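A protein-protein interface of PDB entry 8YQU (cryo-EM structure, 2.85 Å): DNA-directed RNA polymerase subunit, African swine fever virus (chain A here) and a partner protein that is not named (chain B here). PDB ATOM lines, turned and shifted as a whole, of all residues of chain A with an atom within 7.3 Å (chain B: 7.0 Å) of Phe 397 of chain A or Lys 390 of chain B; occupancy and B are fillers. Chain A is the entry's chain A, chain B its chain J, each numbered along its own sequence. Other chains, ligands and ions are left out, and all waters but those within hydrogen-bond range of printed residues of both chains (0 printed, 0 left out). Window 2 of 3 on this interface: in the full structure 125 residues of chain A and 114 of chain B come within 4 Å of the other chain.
The backbone carbonyl oxygen of Lys 394 of chain A sits at hydrogen-bond distance from the side-chain amino group of Lys 336 of chain B (3.1 Å). NZ of Lys 336 of chain B sits at hydrogen-bond distance from O of Asp 396 of chain A (3.2 Å). O of Phe 397 of chain A lies within hydrogen-bond range of NE2 of Gln 333 of chain B (2.9 Å).
The side-chain amide nitrogen (NE2) of Gln 395 of chain A is in hydrogen-bond range of the side-chain carboxylate (OD1) of Asp 396 of chain A (2.5 Å). The side-chain hydroxyl (OH) of Tyr 386 of chain B lies within hydrogen-bond range of the side-chain amide oxygen (OE1) of Gln 330 of chain B (2.9 Å).
CG of Met 363 of chain A touches CG2 of Thr 329 of chain B, 3.5 Å away. Met 363 of chain A touches Gln 333 of chain B. Leu 367 of chain A touches Thr 329 of chain B. Gln 333 of chain B touches Leu 367 of chain A (NE2 to CD2, 3.3 Å). Asp 396 of chain A touches Trp 393 of chain B. Phe 397 of chain A touches Ile 389 of chain B (CD1 to CG2, 3.4 Å). Lys 390 of chain B touches Phe 397 of chain A (CB to CE2, 3.8 Å). Phe 397 of chain A touches Trp 393 of chain B (CB to CG, 3.6 Å). O of Arg 398 of chain A touches CZ2 of Trp 393 of chain B, 3.2 Å away. Trp 393 of chain B touches Glu 400 of chain A.
Of the printed residues of chain B, Leu 367 of chain A touches Thr 329 (3.8 Å) and Gln 333 (3.3 Å). Phe 397 of chain A touches just these residues of chain B: Gln 333 (2.9 Å), Tyr 386 (3.5 Å), Ile 389 (3.4 Å), Lys 390 (3.8 Å) and Trp 393 (3.6 Å). Printed residues of chain A within 4 Å of Lys 336 of chain B: Lys 394 (3.1 Å) and Asp 396 (3.2 Å). Thr 384 of chain B touches none of the printed residues of chain A. Printed residues of chain A within 4 Å of Lys 390 of chain B: Phe 397. Gln 396 of chain B touches none of the printed residues of chain A. The nearest residue of chain B that does not touch Phe 397 of chain A is Lys 336 of chain B (4.8 Å). The nearest printed residue of chain B that does not touch Arg 398 of chain A is Thr 329 of chain B (4.5 Å).
Printed residues of chain A that touch a printed residue of chain B: Met 363, Leu 367, Lys 394, Asp 396, Phe 397, Arg 398 and Glu 400. Hydrophobic or aromatic side chains of chain A within 4 Å of the printed part of chain B: Met 363, Leu 367 and Phe 397. Printed residues of chain B that touch a printed residue of chain A: Thr 329, Gln 333, Lys 336, Tyr 386, Ile 389, Lys 390 and Trp 393. Hydrophobic or aromatic side chains of chain B within 4 Å of the printed part of chain A: Tyr 386, Ile 389 and Trp 393. Among the printed residues, no Asp or Glu carboxylate lies within 4 Å of a Lys or Arg side-chain nitrogen of the other chain.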
ATOM      1  N   MET A 363      15.322  23.467 -19.282  1.00  0.00           N
ATOM      2  CA  MET A 363      14.134  22.720 -19.691  1.00  0.00           C
ATOM      3  C   MET A 363      14.271  22.075 -21.067  1.00  0.00           C
ATOM      4  O   MET A 363      13.861  20.911 -21.215  1.00  0.00           O
ATOM      5  CB  MET A 363      12.908  23.633 -19.611  1.00  0.00           C
ATOM      6  CG  MET A 363      11.614  22.895 -19.819  1.00  0.00           C
ATOM      7  SD  MET A 363      11.321  21.735 -18.478  1.00  0.00           S
ATOM      8  CE  MET A 363      10.251  20.570 -19.305  1.00  0.00           C
ATOM      9  N   PHE A 366      15.868  18.784 -20.726  1.00  0.00           N
ATOM     10  CA  PHE A 366      15.019  17.758 -20.130  1.00  0.00           C
ATOM     11  C   PHE A 366      14.139  17.081 -21.172  1.00  0.00           C
ATOM     12  O   PHE A 366      13.989  15.854 -21.168  1.00  0.00           O
ATOM     13  CB  PHE A 366      14.158  18.382 -19.033  1.00  0.00           C
ATOM     14  CG  PHE A 366      13.169  17.436 -18.416  1.00  0.00           C
ATOM     15  CD1 PHE A 366      13.579  16.464 -17.522  1.00  0.00           C
ATOM     16  CD2 PHE A 366      11.824  17.529 -18.724  1.00  0.00           C
ATOM     17  CE1 PHE A 366      12.662  15.607 -16.947  1.00  0.00           C
ATOM     18  CE2 PHE A 366      10.906  16.671 -18.158  1.00  0.00           C
ATOM     19  CZ  PHE A 366      11.327  15.707 -17.269  1.00  0.00           C
ATOM     20  N   LEU A 367      13.547  17.865 -22.072  1.00  0.00           N
ATOM     21  CA  LEU A 367      12.584  17.328 -23.023  1.00  0.00           C
ATOM     22  C   LEU A 367      13.229  16.494 -24.120  1.00  0.00           C
ATOM     23  O   LEU A 367      12.547  15.658 -24.721  1.00  0.00           O
ATOM     24  CB  LEU A 367      11.778  18.471 -23.641  1.00  0.00           C
ATOM     25  CG  LEU A 367      10.844  19.165 -22.648  1.00  0.00           C
ATOM     26  CD1 LEU A 367      10.288  20.458 -23.216  1.00  0.00           C
ATOM     27  CD2 LEU A 367       9.721  18.226 -22.243  1.00  0.00           C
ATOM     28  N   LYS A 394       8.552  10.244 -18.046  1.00  0.00           N
ATOM     29  CA  LYS A 394       8.120  11.164 -19.092  1.00  0.00           C
ATOM     30  C   LYS A 394       6.741  11.744 -18.798  1.00  0.00           C
ATOM     31  O   LYS A 394       6.100  12.292 -19.701  1.00  0.00           O
ATOM     32  CB  LYS A 394       8.124  10.470 -20.456  1.00  0.00           C
ATOM     33  CG  LYS A 394       9.515  10.190 -21.002  1.00  0.00           C
ATOM     34  CD  LYS A 394       9.515  10.122 -22.520  1.00  0.00           C
ATOM     35  CE  LYS A 394       9.356  11.501 -23.135  1.00  0.00           C
ATOM     36  NZ  LYS A 394       8.818  11.427 -24.521  1.00  0.00           N
ATOM     37  N   GLN A 395       6.272  11.636 -17.557  1.00  0.00           N
ATOM     38  CA  GLN A 395       4.953  12.109 -17.168  1.00  0.00           C
ATOM     39  C   GLN A 395       4.985  13.471 -16.483  1.00  0.00           C
ATOM     40  O   GLN A 395       3.937  13.953 -16.039  1.00  0.00           O
ATOM     41  CB  GLN A 395       4.274  11.071 -16.267  1.00  0.00           C
ATOM     42  CG  GLN A 395       5.000  10.778 -14.955  1.00  0.00           C
ATOM     43  CD  GLN A 395       4.667  11.766 -13.853  1.00  0.00           C
ATOM     44  OE1 GLN A 395       3.573  12.326 -13.814  1.00  0.00           O
ATOM     45  NE2 GLN A 395       5.615  11.982 -12.949  1.00  0.00           N
ATOM     46  N   ASP A 396       6.149  14.108 -16.397  1.00  0.00           N
ATOM     47  CA  ASP A 396       6.287  15.398 -15.736  1.00  0.00           C
ATOM     48  C   ASP A 396       6.328  16.514 -16.772  1.00  0.00           C
ATOM     49  O   ASP A 396       7.096  16.443 -17.737  1.00  0.00           O
ATOM     50  CB  ASP A 396       7.549  15.438 -14.871  1.00  0.00           C
ATOM     51  CG  ASP A 396       7.451  14.539 -13.656  1.00  0.00           C
ATOM     52  OD1 ASP A 396       6.324  14.326 -13.162  1.00  0.00           O
ATOM     53  OD2 ASP A 396       8.501  14.051 -13.190  1.00  0.00           O
ATOM     54  N   PHE A 397       5.497  17.540 -16.569  1.00  0.00           N
ATOM     55  CA  PHE A 397       5.516  18.694 -17.461  1.00  0.00           C
ATOM     56  C   PHE A 397       6.833  19.453 -17.364  1.00  0.00           C
ATOM     57  O   PHE A 397       7.419  19.819 -18.388  1.00  0.00           O
ATOM     58  CB  PHE A 397       4.342  19.621 -17.151  1.00  0.00           C
ATOM     59  CG  PHE A 397       3.999  20.557 -18.274  1.00  0.00           C
ATOM     60  CD1 PHE A 397       3.551  20.073 -19.490  1.00  0.00           C
ATOM     61  CD2 PHE A 397       4.121  21.926 -18.109  1.00  0.00           C
ATOM     62  CE1 PHE A 397       3.236  20.936 -20.522  1.00  0.00           C
ATOM     63  CE2 PHE A 397       3.808  22.793 -19.135  1.00  0.00           C
ATOM     64  CZ  PHE A 397       3.365  22.298 -20.343  1.00  0.00           C
ATOM     65  N   ARG A 398       7.307  19.710 -16.148  1.00  0.00           N
ATOM     66  CA  ARG A 398       8.565  20.414 -15.927  1.00  0.00           C
ATOM     67  C   ARG A 398       9.288  19.751 -14.761  1.00  0.00           C
ATOM     68  O   ARG A 398       8.958  18.632 -14.352  1.00  0.00           O
ATOM     69  CB  ARG A 398       8.342  21.913 -15.674  1.00  0.00           C
ATOM     70  CG  ARG A 398       7.500  22.626 -16.715  1.00  0.00           C
ATOM     71  CD  ARG A 398       7.018  23.972 -16.202  1.00  0.00           C
ATOM     72  NE  ARG A 398       8.122  24.913 -16.044  1.00  0.00           N
ATOM     73  CZ  ARG A 398       8.701  25.565 -17.043  1.00  0.00           C
ATOM     74  NH1 ARG A 398       8.303  25.407 -18.295  1.00  0.00           N
ATOM     75  NH2 ARG A 398       9.705  26.396 -16.779  1.00  0.00           N
ATOM     76  N   LEU A 399      10.287  20.445 -14.226  1.00  0.00           N
ATOM     77  CA  LEU A 399      11.106  19.932 -13.141  1.00  0.00           C
ATOM     78  C   LEU A 399      10.773  20.650 -11.840  1.00  0.00           C
ATOM     79  O   LEU A 399      10.273  21.777 -11.830  1.00  0.00           O
ATOM     80  CB  LEU A 399      12.597  20.100 -13.451  1.00  0.00           C
ATOM     81  CG  LEU A 399      13.228  19.134 -14.455  1.00  0.00           C
ATOM     82  CD1 LEU A 399      12.773  19.477 -15.857  1.00  0.00           C
ATOM     83  CD2 LEU A 399      14.743  19.148 -14.368  1.00  0.00           C
ATOM     84  N   GLU A 400      11.059  19.976 -10.732  1.00  0.00           N
ATOM     85  CA  GLU A 400      10.881  20.557  -9.414  1.00  0.00           C
ATOM     86  C   GLU A 400      12.144  21.299  -8.994  1.00  0.00           C
ATOM     87  O   GLU A 400      13.265  20.866  -9.275  1.00  0.00           O
ATOM     88  CB  GLU A 400      10.538  19.480  -8.384  1.00  0.00           C
ATOM     89  CG  GLU A 400       9.180  18.822  -8.591  1.00  0.00           C
ATOM     90  CD  GLU A 400       9.215  17.704  -9.616  1.00  0.00           C
ATOM     91  OE1 GLU A 400      10.311  17.393 -10.126  1.00  0.00           O
ATOM     92  OE2 GLU A 400       8.143  17.134  -9.910  1.00  0.00           O
ATOM     93  N   THR B 329      11.052  25.393 -25.897  1.00  0.00           N
ATOM     94  CA  THR B 329      10.382  24.599 -24.872  1.00  0.00           C
ATOM     95  C   THR B 329       8.947  24.279 -25.271  1.00  0.00           C
ATOM     96  O   THR B 329       8.496  23.132 -25.150  1.00  0.00           O
ATOM     97  CB  THR B 329      10.409  25.340 -23.536  1.00  0.00           C
ATOM     98  OG1 THR B 329      11.758  25.687 -23.202  1.00  0.00           O
ATOM     99  CG2 THR B 329       9.819  24.475 -22.438  1.00  0.00           C
ATOM    100  N   GLN B 330       8.210  25.286 -25.747  1.00  0.00           N
ATOM    101  CA  GLN B 330       6.822  25.050 -26.132  1.00  0.00           C
ATOM    102  C   GLN B 330       6.733  24.085 -27.308  1.00  0.00           C
ATOM    103  O   GLN B 330       5.856  23.212 -27.340  1.00  0.00           O
ATOM    104  CB  GLN B 330       6.133  26.372 -26.463  1.00  0.00           C
ATOM    105  CG  GLN B 330       4.615  26.298 -26.402  1.00  0.00           C
ATOM    106  CD  GLN B 330       3.973  27.648 -26.165  1.00  0.00           C
ATOM    107  OE1 GLN B 330       3.680  28.018 -25.028  1.00  0.00           O
ATOM    108  NE2 GLN B 330       3.749  28.394 -27.241  1.00  0.00           N
ATOM    109  N   GLN B 333       7.367  20.581 -26.054  1.00  0.00           N
ATOM    110  CA  GLN B 333       6.172  20.093 -25.369  1.00  0.00           C
ATOM    111  C   GLN B 333       5.111  19.650 -26.370  1.00  0.00           C
ATOM    112  O   GLN B 333       4.492  18.586 -26.210  1.00  0.00           O
ATOM    113  CB  GLN B 333       5.613  21.179 -24.448  1.00  0.00           C
ATOM    114  CG  GLN B 333       6.410  21.409 -23.175  1.00  0.00           C
ATOM    115  CD  GLN B 333       6.325  20.242 -22.211  1.00  0.00           C
ATOM    116  OE1 GLN B 333       5.434  19.398 -22.313  1.00  0.00           O
ATOM    117  NE2 GLN B 333       7.245  20.196 -21.256  1.00  0.00           N
ATOM    118  N   LYS B 336       6.208  16.350 -27.896  1.00  0.00           N
ATOM    119  CA  LYS B 336       6.094  15.261 -26.931  1.00  0.00           C
ATOM    120  C   LYS B 336       4.648  14.806 -26.793  1.00  0.00           C
ATOM    121  O   LYS B 336       4.363  13.603 -26.719  1.00  0.00           O
ATOM    122  CB  LYS B 336       6.655  15.704 -25.579  1.00  0.00           C
ATOM    123  CG  LYS B 336       6.408  14.723 -24.449  1.00  0.00           C
ATOM    124  CD  LYS B 336       6.841  15.308 -23.118  1.00  0.00           C
ATOM    125  CE  LYS B 336       6.249  14.531 -21.957  1.00  0.00           C
ATOM    126  NZ  LYS B 336       6.549  15.176 -20.651  1.00  0.00           N
ATOM    127  N   ILE B 337       3.715  15.758 -26.758  1.00  0.00           N
ATOM    128  CA  ILE B 337       2.304  15.388 -26.677  1.00  0.00           C
ATOM    129  C   ILE B 337       1.848  14.722 -27.972  1.00  0.00           C
ATOM    130  O   ILE B 337       1.050  13.777 -27.952  1.00  0.00           O
ATOM    131  CB  ILE B 337       1.457  16.621 -26.320  1.00  0.00           C
ATOM    132  CG1 ILE B 337       1.678  16.966 -24.848  1.00  0.00           C
ATOM    133  CG2 ILE B 337      -0.015  16.367 -26.589  1.00  0.00           C
ATOM    134  CD1 ILE B 337       1.205  18.324 -24.462  1.00  0.00           C
ATOM    135  N   THR B 384      -5.151  22.202 -26.832  1.00  0.00           N
ATOM    136  CA  THR B 384      -5.937  22.347 -25.610  1.00  0.00           C
ATOM    137  C   THR B 384      -5.464  21.386 -24.527  1.00  0.00           C
ATOM    138  O   THR B 384      -5.481  21.721 -23.339  1.00  0.00           O
ATOM    139  CB  THR B 384      -7.426  22.135 -25.897  1.00  0.00           C
ATOM    140  OG1 THR B 384      -7.669  20.757 -26.210  1.00  0.00           O
ATOM    141  CG2 THR B 384      -7.894  23.026 -27.039  1.00  0.00           C
ATOM    142  N   GLU B 385      -5.021  20.190 -24.915  1.00  0.00           N
ATOM    143  CA  GLU B 385      -4.571  19.213 -23.933  1.00  0.00           C
ATOM    144  C   GLU B 385      -3.204  19.601 -23.382  1.00  0.00           C
ATOM    145  O   GLU B 385      -2.900  19.338 -22.214  1.00  0.00           O
ATOM    146  CB  GLU B 385      -4.556  17.826 -24.582  1.00  0.00           C
ATOM    147  CG  GLU B 385      -4.427  16.637 -23.643  1.00  0.00           C
ATOM    148  CD  GLU B 385      -3.005  16.317 -23.259  1.00  0.00           C
ATOM    149  OE1 GLU B 385      -2.085  16.620 -24.045  1.00  0.00           O
ATOM    150  OE2 GLU B 385      -2.819  15.719 -22.180  1.00  0.00           O
ATOM    151  N   TYR B 386      -2.378  20.255 -24.203  1.00  0.00           N
ATOM    152  CA  TYR B 386      -1.141  20.849 -23.707  1.00  0.00           C
ATOM    153  C   TYR B 386      -1.434  21.909 -22.656  1.00  0.00           C
ATOM    154  O   TYR B 386      -0.813  21.935 -21.586  1.00  0.00           O
ATOM    155  CB  TYR B 386      -0.347  21.456 -24.866  1.00  0.00           C
ATOM    156  CG  TYR B 386       0.573  22.589 -24.459  1.00  0.00           C
ATOM    157  CD1 TYR B 386       1.834  22.332 -23.938  1.00  0.00           C
ATOM    158  CD2 TYR B 386       0.181  23.917 -24.598  1.00  0.00           C
ATOM    159  CE1 TYR B 386       2.679  23.363 -23.567  1.00  0.00           C
ATOM    160  CE2 TYR B 386       1.018  24.952 -24.228  1.00  0.00           C
ATOM    161  CZ  TYR B 386       2.265  24.669 -23.713  1.00  0.00           C
ATOM    162  OH  TYR B 386       3.101  25.698 -23.344  1.00  0.00           O
ATOM    163  N   LEU B 387      -2.381  22.802 -22.954  1.00  0.00           N
ATOM    164  CA  LEU B 387      -2.761  23.812 -21.972  1.00  0.00           C
ATOM    165  C   LEU B 387      -3.343  23.180 -20.711  1.00  0.00           C
ATOM    166  O   LEU B 387      -3.097  23.676 -19.606  1.00  0.00           O
ATOM    167  CB  LEU B 387      -3.756  24.796 -22.587  1.00  0.00           C
ATOM    168  CG  LEU B 387      -4.187  25.963 -21.698  1.00  0.00           C
ATOM    169  CD1 LEU B 387      -2.989  26.828 -21.345  1.00  0.00           C
ATOM    170  CD2 LEU B 387      -5.259  26.790 -22.386  1.00  0.00           C
ATOM    171  N   ASN B 388      -4.093  22.088 -20.857  1.00  0.00           N
ATOM    172  CA  ASN B 388      -4.638  21.378 -19.706  1.00  0.00           C
ATOM    173  C   ASN B 388      -3.532  20.786 -18.838  1.00  0.00           C
ATOM    174  O   ASN B 388      -3.589  20.877 -17.608  1.00  0.00           O
ATOM    175  CB  ASN B 388      -5.597  20.283 -20.175  1.00  0.00           C
ATOM    176  CG  ASN B 388      -7.050  20.704 -20.086  1.00  0.00           C
ATOM    177  OD1 ASN B 388      -7.510  21.171 -19.044  1.00  0.00           O
ATOM    178  ND2 ASN B 388      -7.781  20.541 -21.182  1.00  0.00           N
ATOM    179  N   ILE B 389      -2.523  20.168 -19.460  1.00  0.00           N
ATOM    180  CA  ILE B 389      -1.404  19.633 -18.684  1.00  0.00           C
ATOM    181  C   ILE B 389      -0.643  20.757 -17.998  1.00  0.00           C
ATOM    182  O   ILE B 389      -0.184  20.600 -16.861  1.00  0.00           O
ATOM    183  CB  ILE B 389      -0.464  18.787 -19.565  1.00  0.00           C
ATOM    184  CG1 ILE B 389      -1.200  17.597 -20.172  1.00  0.00           C
ATOM    185  CG2 ILE B 389       0.710  18.276 -18.747  1.00  0.00           C
ATOM    186  CD1 ILE B 389      -0.261  16.542 -20.726  1.00  0.00           C
ATOM    187  N   LYS B 390      -0.487  21.899 -18.671  1.00  0.00           N
ATOM    188  CA  LYS B 390       0.167  23.040 -18.038  1.00  0.00           C
ATOM    189  C   LYS B 390      -0.608  23.498 -16.807  1.00  0.00           C
ATOM    190  O   LYS B 390      -0.023  23.767 -15.750  1.00  0.00           O
ATOM    191  CB  LYS B 390       0.314  24.182 -19.043  1.00  0.00           C
ATOM    192  CG  LYS B 390       1.059  25.393 -18.511  1.00  0.00           C
ATOM    193  CD  LYS B 390       1.211  26.458 -19.583  1.00  0.00           C
ATOM    194  CE  LYS B 390       2.030  27.635 -19.083  1.00  0.00           C
ATOM    195  NZ  LYS B 390       1.313  28.391 -18.019  1.00  0.00           N
ATOM    196  N   LYS B 391      -1.936  23.578 -16.925  1.00  0.00           N
ATOM    197  CA  LYS B 391      -2.760  23.966 -15.785  1.00  0.00           C
ATOM    198  C   LYS B 391      -2.660  22.949 -14.654  1.00  0.00           C
ATOM    199  O   LYS B 391      -2.593  23.323 -13.477  1.00  0.00           O
ATOM    200  CB  LYS B 391      -4.214  24.137 -16.224  1.00  0.00           C
ATOM    201  CG  LYS B 391      -5.141  24.609 -15.118  1.00  0.00           C
ATOM    202  CD  LYS B 391      -6.344  25.343 -15.683  1.00  0.00           C
ATOM    203  CE  LYS B 391      -7.039  26.167 -14.612  1.00  0.00           C
ATOM    204  NZ  LYS B 391      -8.406  26.581 -15.032  1.00  0.00           N
ATOM    205  N   GLN B 392      -2.657  21.656 -14.989  1.00  0.00           N
ATOM    206  CA  GLN B 392      -2.544  20.623 -13.964  1.00  0.00           C
ATOM    207  C   GLN B 392      -1.200  20.697 -13.251  1.00  0.00           C
ATOM    208  O   GLN B 392      -1.129  20.528 -12.028  1.00  0.00           O
ATOM    209  CB  GLN B 392      -2.745  19.238 -14.581  1.00  0.00           C
ATOM    210  CG  GLN B 392      -4.128  19.005 -15.169  1.00  0.00           C
ATOM    211  CD  GLN B 392      -5.218  19.002 -14.118  1.00  0.00           C
ATOM    212  OE1 GLN B 392      -5.033  18.485 -13.016  1.00  0.00           O
ATOM    213  NE2 GLN B 392      -6.366  19.579 -14.454  1.00  0.00           N
ATOM    214  N   TRP B 393      -0.122  20.940 -13.999  1.00  0.00           N
ATOM    215  CA  TRP B 393       1.189  21.080 -13.376  1.00  0.00           C
ATOM    216  C   TRP B 393       1.243  22.312 -12.481  1.00  0.00           C
ATOM    217  O   TRP B 393       1.846  22.276 -11.403  1.00  0.00           O
ATOM    218  CB  TRP B 393       2.282  21.143 -14.443  1.00  0.00           C
ATOM    219  CG  TRP B 393       3.661  21.046 -13.871  1.00  0.00           C
ATOM    220  CD1 TRP B 393       4.545  22.066 -13.679  1.00  0.00           C
ATOM    221  CD2 TRP B 393       4.313  19.858 -13.406  1.00  0.00           C
ATOM    222  NE1 TRP B 393       5.709  21.588 -13.128  1.00  0.00           N
ATOM    223  CE2 TRP B 393       5.591  20.234 -12.950  1.00  0.00           C
ATOM    224  CE3 TRP B 393       3.940  18.512 -13.334  1.00  0.00           C
ATOM    225  CZ2 TRP B 393       6.497  19.314 -12.429  1.00  0.00           C
ATOM    226  CZ3 TRP B 393       4.841  17.602 -12.816  1.00  0.00           C
ATOM    227  CH2 TRP B 393       6.104  18.006 -12.371  1.00  0.00           C
ATOM    228  N   GLU B 394       0.620  23.412 -12.912  1.00  0.00           N
ATOM    229  CA  GLU B 394       0.565  24.597 -12.063  1.00  0.00           C
ATOM    230  C   GLU B 394      -0.209  24.314 -10.780  1.00  0.00           C
ATOM    231  O   GLU B 394       0.187  24.755  -9.694  1.00  0.00           O
ATOM    232  CB  GLU B 394      -0.061  25.763 -12.828  1.00  0.00           C
ATOM    233  CG  GLU B 394      -0.209  27.045 -12.019  1.00  0.00           C
ATOM    234  CD  GLU B 394       0.999  27.336 -11.145  1.00  0.00           C
ATOM    235  OE1 GLU B 394       2.138  27.291 -11.660  1.00  0.00           O
ATOM    236  OE2 GLU B 394       0.811  27.610  -9.943  1.00  0.00           O
ATOM    237  N   LEU B 395      -1.317  23.578 -10.887  1.00  0.00           N
ATOM    238  CA  LEU B 395      -2.079  23.206  -9.699  1.00  0.00           C
ATOM    239  C   LEU B 395      -1.254  22.324  -8.769  1.00  0.00           C
ATOM    240  O   LEU B 395      -1.310  22.476  -7.543  1.00  0.00           O
ATOM    241  CB  LEU B 395      -3.371  22.495 -10.105  1.00  0.00           C
ATOM    242  CG  LEU B 395      -4.482  23.375 -10.678  1.00  0.00           C
ATOM    243  CD1 LEU B 395      -5.758  22.569 -10.867  1.00  0.00           C
ATOM    244  CD2 LEU B 395      -4.730  24.580  -9.785  1.00  0.00           C
ATOM    245  N   GLN B 396      -0.490  21.387  -9.336  1.00  0.00           N
ATOM    246  CA  GLN B 396       0.384  20.546  -8.523  1.00  0.00           C
ATOM    247  C   GLN B 396       1.453  21.379  -7.828  1.00  0.00           C
ATOM    248  O   GLN B 396       1.833  21.090  -6.687  1.00  0.00           O
ATOM    249  CB  GLN B 396       1.024  19.461  -9.388  1.00  0.00           C
ATOM    250  CG  GLN B 396       1.358  18.186  -8.634  1.00  0.00           C
ATOM    251  CD  GLN B 396       1.993  17.134  -9.522  1.00  0.00           C
ATOM    252  OE1 GLN B 396       1.729  17.078 -10.723  1.00  0.00           O
ATOM    253  NE2 GLN B 396       2.832  16.290  -8.933  1.00  0.00           N
